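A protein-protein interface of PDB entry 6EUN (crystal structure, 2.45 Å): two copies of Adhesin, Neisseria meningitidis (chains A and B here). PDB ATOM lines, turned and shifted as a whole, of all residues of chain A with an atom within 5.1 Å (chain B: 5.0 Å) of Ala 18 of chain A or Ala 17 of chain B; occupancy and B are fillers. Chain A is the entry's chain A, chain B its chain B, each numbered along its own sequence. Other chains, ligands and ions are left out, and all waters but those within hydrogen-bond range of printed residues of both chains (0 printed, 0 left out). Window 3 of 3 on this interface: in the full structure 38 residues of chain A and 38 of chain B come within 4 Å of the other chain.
Ile 15 of chain A touches Ala 14 of chain B, but with the chains exchanged Ala 14 of chain A does not touch Ile 15 of chain B (6.2 Å). Ala 18 of chain A touches Ala 17 of chain B, but with the chains exchanged Ala 17 of chain A does not touch Ala 18 of chain B (7.4 Å). Ala 18 of chain A touches Asn 21 of chain B, but with the chains exchanged Asn 21 of chain A does not touch Ala 18 of chain B (6.7 Å). Asn 21 of chain A touches its own counterpart, Asn 21 of chain B. Positions printed for both chains: 13, 14, 15, 16, 17, 18, 19, 20 and 21. Of the 7 pairs that touch across the chains among the printed residues, 2 have their exchanged pair printed and touching as well.
The backbone carbonyl oxygen (O) of Ala 18 of chain A sits at hydrogen-bond distance from the side-chain amide nitrogen (ND2) of Asn 21 of chain B (2.9 Å).
Hydrophobic or aromatic side chains of chain B that line the printed part of chain A: Val 13, Ala 14 and Ala 17. Among the printed residues, 7 pairs touch across the chains.
Of chain B, only Ala 17 (3.6 Å) and Asn 21 (2.9 Å) come within 4 Å of Ala 18 of chain A. Of the printed residues of chain B, Asn 21 of chain A touches Asn 21 (3.8 Å). Printed residues of chain B within 4 Å of Ile 15 of chain A: Val 13 and Ala 14. Ile 15 of chain B touches none of the printed residues of chain A. Ile 37 of chain B touches none of the printed residues of chain A. The nearest printed residue of chain A that does not touch Ala 17 of chain B is Tyr 19 of chain A (5.5 Å). The nearest printed residue of chain A that does not touch Ala 14 of chain B is Ala 18 of chain A (4.4 Å).
CB of Ala 14 of chain A touches CB of Ala 14 of chain B (3.7 Å). Val 13 of chain B touches Ile 15 of chain A (CB to CD1, 3.6 Å). Ala 14 of chain B touches Ile 15 of chain A (N to CD1, 3.4 Å). CB of Ala 17 of chain B touches CB of Ala 18 of chain A (3.6 Å). Asn 21 of chain B touches Asn 21 of chain A (ND2 to CB, 3.8 Å). Asn 21 of chain B touches Gly 22 of chain A.
O of Ala 17 of chain A sits close to ND2 of Asn 21 of chain A (3.4 Å). The backbone carbonyl oxygen of Ala 17 of chain B lies close to the side-chain amide nitrogen of Asn 21 of chain B, 3.4 Å away.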
ATOM      1  N   VAL A  13     -21.103 -26.447 -18.499  1.00  0.00           N
ATOM      2  CA  VAL A  13     -21.255 -26.845 -17.095  1.00  0.00           C
ATOM      3  C   VAL A  13     -19.864 -26.980 -16.462  1.00  0.00           C
ATOM      4  O   VAL A  13     -19.644 -26.447 -15.379  1.00  0.00           O
ATOM      5  CB  VAL A  13     -22.109 -28.129 -16.895  1.00  0.00           C
ATOM      6  CG1 VAL A  13     -22.272 -28.463 -15.410  1.00  0.00           C
ATOM      7  CG2 VAL A  13     -23.475 -28.004 -17.550  1.00  0.00           C
ATOM      8  N   ALA A  14     -18.928 -27.652 -17.167  1.00  0.00           N
ATOM      9  CA  ALA A  14     -17.553 -27.895 -16.744  1.00  0.00           C
ATOM     10  C   ALA A  14     -16.797 -26.605 -16.474  1.00  0.00           C
ATOM     11  O   ALA A  14     -16.129 -26.528 -15.450  1.00  0.00           O
ATOM     12  CB  ALA A  14     -16.832 -28.727 -17.783  1.00  0.00           C
ATOM     13  N   ILE A  15     -16.936 -25.581 -17.346  1.00  0.00           N
ATOM     14  CA  ILE A  15     -16.314 -24.260 -17.180  1.00  0.00           C
ATOM     15  C   ILE A  15     -16.849 -23.606 -15.903  1.00  0.00           C
ATOM     16  O   ILE A  15     -16.058 -23.155 -15.074  1.00  0.00           O
ATOM     17  CB  ILE A  15     -16.556 -23.362 -18.433  1.00  0.00           C
ATOM     18  CG1 ILE A  15     -15.604 -23.720 -19.592  1.00  0.00           C
ATOM     19  CG2 ILE A  15     -16.502 -21.849 -18.111  1.00  0.00           C
ATOM     20  CD1 ILE A  15     -14.165 -23.264 -19.405  1.00  0.00           C
ATOM     21  N   ALA A  16     -18.191 -23.574 -15.748  1.00  0.00           N
ATOM     22  CA  ALA A  16     -18.903 -22.999 -14.611  1.00  0.00           C
ATOM     23  C   ALA A  16     -18.519 -23.705 -13.312  1.00  0.00           C
ATOM     24  O   ALA A  16     -18.240 -23.037 -12.321  1.00  0.00           O
ATOM     25  CB  ALA A  16     -20.402 -23.092 -14.845  1.00  0.00           C
ATOM     26  N   ALA A  17     -18.443 -25.048 -13.335  1.00  0.00           N
ATOM     27  CA  ALA A  17     -18.073 -25.863 -12.187  1.00  0.00           C
ATOM     28  C   ALA A  17     -16.627 -25.605 -11.765  1.00  0.00           C
ATOM     29  O   ALA A  17     -16.378 -25.445 -10.564  1.00  0.00           O
ATOM     30  CB  ALA A  17     -18.289 -27.336 -12.495  1.00  0.00           C
ATOM     31  N   ALA A  18     -15.682 -25.536 -12.750  1.00  0.00           N
ATOM     32  CA  ALA A  18     -14.260 -25.279 -12.511  1.00  0.00           C
ATOM     33  C   ALA A  18     -14.069 -23.870 -11.974  1.00  0.00           C
ATOM     34  O   ALA A  18     -13.271 -23.657 -11.054  1.00  0.00           O
ATOM     35  CB  ALA A  18     -13.460 -25.485 -13.781  1.00  0.00           C
ATOM     36  N   TYR A  19     -14.861 -22.924 -12.504  1.00  0.00           N
ATOM     37  CA  TYR A  19     -14.870 -21.532 -12.060  1.00  0.00           C
ATOM     38  C   TYR A  19     -15.279 -21.460 -10.565  1.00  0.00           C
ATOM     39  O   TYR A  19     -14.555 -20.849  -9.774  1.00  0.00           O
ATOM     40  CB  TYR A  19     -15.815 -20.696 -12.942  1.00  0.00           C
ATOM     41  CG  TYR A  19     -15.858 -19.231 -12.562  1.00  0.00           C
ATOM     42  CD1 TYR A  19     -16.713 -18.772 -11.557  1.00  0.00           C
ATOM     43  CD2 TYR A  19     -15.040 -18.301 -13.197  1.00  0.00           C
ATOM     44  CE1 TYR A  19     -16.756 -17.427 -11.201  1.00  0.00           C
ATOM     45  CE2 TYR A  19     -15.074 -16.951 -12.851  1.00  0.00           C
ATOM     46  CZ  TYR A  19     -15.934 -16.519 -11.850  1.00  0.00           C
ATOM     47  OH  TYR A  19     -15.963 -15.190 -11.502  1.00  0.00           O
ATOM     48  N   ASN A  20     -16.420 -22.110 -10.186  1.00  0.00           N
ATOM     49  CA  ASN A  20     -16.914 -22.180  -8.806  1.00  0.00           C
ATOM     50  C   ASN A  20     -15.894 -22.815  -7.870  1.00  0.00           C
ATOM     51  O   ASN A  20     -15.645 -22.264  -6.795  1.00  0.00           O
ATOM     52  CB  ASN A  20     -18.240 -22.946  -8.700  1.00  0.00           C
ATOM     53  CG  ASN A  20     -19.470 -22.163  -9.102  1.00  0.00           C
ATOM     54  OD1 ASN A  20     -19.443 -20.930  -9.304  1.00  0.00           O
ATOM     55  ND2 ASN A  20     -20.589 -22.876  -9.218  1.00  0.00           N
ATOM     56  N   ASN A  21     -15.308 -23.964  -8.262  1.00  0.00           N
ATOM     57  CA  ASN A  21     -14.324 -24.610  -7.411  1.00  0.00           C
ATOM     58  C   ASN A  21     -13.138 -23.681  -7.129  1.00  0.00           C
ATOM     59  O   ASN A  21     -12.701 -23.592  -5.971  1.00  0.00           O
ATOM     60  CB  ASN A  21     -13.873 -25.922  -8.003  1.00  0.00           C
ATOM     61  CG  ASN A  21     -14.903 -27.006  -7.937  1.00  0.00           C
ATOM     62  OD1 ASN A  21     -15.748 -27.036  -7.040  1.00  0.00           O
ATOM     63  ND2 ASN A  21     -14.801 -27.968  -8.846  1.00  0.00           N
ATOM     64  N   GLY A  22     -12.706 -22.946  -8.166  1.00  0.00           N
ATOM     65  CA  GLY A  22     -11.629 -21.964  -8.086  1.00  0.00           C
ATOM     66  C   GLY A  22     -11.916 -20.878  -7.068  1.00  0.00           C
ATOM     67  O   GLY A  22     -11.008 -20.435  -6.375  1.00  0.00           O
ATOM     68  N   VAL B  13     -10.321 -25.105 -21.937  1.00  0.00           N
ATOM     69  CA  VAL B  13     -10.191 -24.236 -20.763  1.00  0.00           C
ATOM     70  C   VAL B  13     -10.635 -25.006 -19.514  1.00  0.00           C
ATOM     71  O   VAL B  13      -9.921 -24.988 -18.517  1.00  0.00           O
ATOM     72  CB  VAL B  13     -10.935 -22.872 -20.897  1.00  0.00           C
ATOM     73  CG1 VAL B  13     -10.717 -21.990 -19.666  1.00  0.00           C
ATOM     74  CG2 VAL B  13     -10.522 -22.124 -22.161  1.00  0.00           C
ATOM     75  N   ALA B  14     -11.779 -25.714 -19.602  1.00  0.00           N
ATOM     76  CA  ALA B  14     -12.373 -26.511 -18.531  1.00  0.00           C
ATOM     77  C   ALA B  14     -11.437 -27.598 -18.024  1.00  0.00           C
ATOM     78  O   ALA B  14     -11.302 -27.742 -16.811  1.00  0.00           O
ATOM     79  CB  ALA B  14     -13.688 -27.113 -18.996  1.00  0.00           C
ATOM     80  N   ILE B  15     -10.756 -28.322 -18.935  1.00  0.00           N
ATOM     81  CA  ILE B  15      -9.775 -29.365 -18.596  1.00  0.00           C
ATOM     82  C   ILE B  15      -8.614 -28.738 -17.818  1.00  0.00           C
ATOM     83  O   ILE B  15      -8.258 -29.230 -16.751  1.00  0.00           O
ATOM     84  CB  ILE B  15      -9.280 -30.104 -19.888  1.00  0.00           C
ATOM     85  CG1 ILE B  15     -10.301 -31.151 -20.397  1.00  0.00           C
ATOM     86  CG2 ILE B  15      -7.881 -30.730 -19.712  1.00  0.00           C
ATOM     87  CD1 ILE B  15     -10.393 -32.426 -19.558  1.00  0.00           C
ATOM     88  N   ALA B  16      -8.043 -27.645 -18.364  1.00  0.00           N
ATOM     89  CA  ALA B  16      -6.931 -26.887 -17.798  1.00  0.00           C
ATOM     90  C   ALA B  16      -7.295 -26.315 -16.422  1.00  0.00           C
ATOM     91  O   ALA B  16      -6.506 -26.435 -15.484  1.00  0.00           O
ATOM     92  CB  ALA B  16      -6.528 -25.773 -18.753  1.00  0.00           C
ATOM     93  N   ALA B  17      -8.514 -25.759 -16.291  1.00  0.00           N
ATOM     94  CA  ALA B  17      -9.019 -25.192 -15.042  1.00  0.00           C
ATOM     95  C   ALA B  17      -9.194 -26.267 -13.969  1.00  0.00           C
ATOM     96  O   ALA B  17      -8.774 -26.045 -12.834  1.00  0.00           O
ATOM     97  CB  ALA B  17     -10.325 -24.457 -15.285  1.00  0.00           C
ATOM     98  N   ALA B  18      -9.784 -27.438 -14.338  1.00  0.00           N
ATOM     99  CA  ALA B  18     -10.009 -28.568 -13.435  1.00  0.00           C
ATOM    100  C   ALA B  18      -8.673 -29.156 -12.998  1.00  0.00           C
ATOM    101  O   ALA B  18      -8.488 -29.487 -11.817  1.00  0.00           O
ATOM    102  CB  ALA B  18     -10.865 -29.627 -14.115  1.00  0.00           C
ATOM    103  N   TYR B  19      -7.719 -29.209 -13.941  1.00  0.00           N
ATOM    104  CA  TYR B  19      -6.359 -29.683 -13.690  1.00  0.00           C
ATOM    105  C   TYR B  19      -5.688 -28.798 -12.625  1.00  0.00           C
ATOM    106  O   TYR B  19      -5.166 -29.325 -11.633  1.00  0.00           O
ATOM    107  CB  TYR B  19      -5.542 -29.686 -14.997  1.00  0.00           C
ATOM    108  CG  TYR B  19      -4.129 -30.193 -14.828  1.00  0.00           C
ATOM    109  CD1 TYR B  19      -3.100 -29.336 -14.441  1.00  0.00           C
ATOM    110  CD2 TYR B  19      -3.820 -31.534 -15.040  1.00  0.00           C
ATOM    111  CE1 TYR B  19      -1.794 -29.799 -14.282  1.00  0.00           C
ATOM    112  CE2 TYR B  19      -2.515 -32.009 -14.887  1.00  0.00           C
ATOM    113  CZ  TYR B  19      -1.504 -31.137 -14.513  1.00  0.00           C
ATOM    114  OH  TYR B  19      -0.222 -31.617 -14.373  1.00  0.00           O
ATOM    115  N   ASN B  20      -5.717 -27.457 -12.828  1.00  0.00           N
ATOM    116  CA  ASN B  20      -5.130 -26.487 -11.903  1.00  0.00           C
ATOM    117  C   ASN B  20      -5.764 -26.525 -10.510  1.00  0.00           C
ATOM    118  O   ASN B  20      -5.031 -26.471  -9.512  1.00  0.00           O
ATOM    119  CB  ASN B  20      -5.163 -25.080 -12.484  1.00  0.00           C
ATOM    120  CG  ASN B  20      -3.805 -24.434 -12.477  1.00  0.00           C
ATOM    121  OD1 ASN B  20      -2.833 -24.933 -13.077  1.00  0.00           O
ATOM    122  ND2 ASN B  20      -3.700 -23.329 -11.761  1.00  0.00           N
ATOM    123  N   ASN B  21      -7.114 -26.644 -10.433  1.00  0.00           N
ATOM    124  CA  ASN B  21      -7.776 -26.732  -9.139  1.00  0.00           C
ATOM    125  C   ASN B  21      -7.322 -27.992  -8.380  1.00  0.00           C
ATOM    126  O   ASN B  21      -7.040 -27.921  -7.177  1.00  0.00           O
ATOM    127  CB  ASN B  21      -9.276 -26.686  -9.297  1.00  0.00           C
ATOM    128  CG  ASN B  21      -9.804 -25.331  -9.691  1.00  0.00           C
ATOM    129  OD1 ASN B  21      -9.201 -24.286  -9.413  1.00  0.00           O
ATOM    130  ND2 ASN B  21     -10.974 -25.315 -10.318  1.00  0.00           N
ATOM    131  N   ILE B  37      -3.758 -19.978 -17.342  1.00  0.00           N
ATOM    132  CA  ILE B  37      -4.877 -19.538 -18.175  1.00  0.00           C
ATOM    133  C   ILE B  37      -4.962 -18.018 -18.170  1.00  0.00           C
ATOM    134  O   ILE B  37      -5.091 -17.396 -17.111  1.00  0.00           O
ATOM    135  CB  ILE B  37      -6.244 -20.234 -17.865  1.00  0.00           C
ATOM    136  CG1 ILE B  37      -6.092 -21.772 -17.743  1.00  0.00           C
ATOM    137  CG2 ILE B  37      -7.295 -19.869 -18.938  1.00  0.00           C
ATOM    138  CD1 ILE B  37      -7.155 -22.451 -16.920  1.00  0.00           C
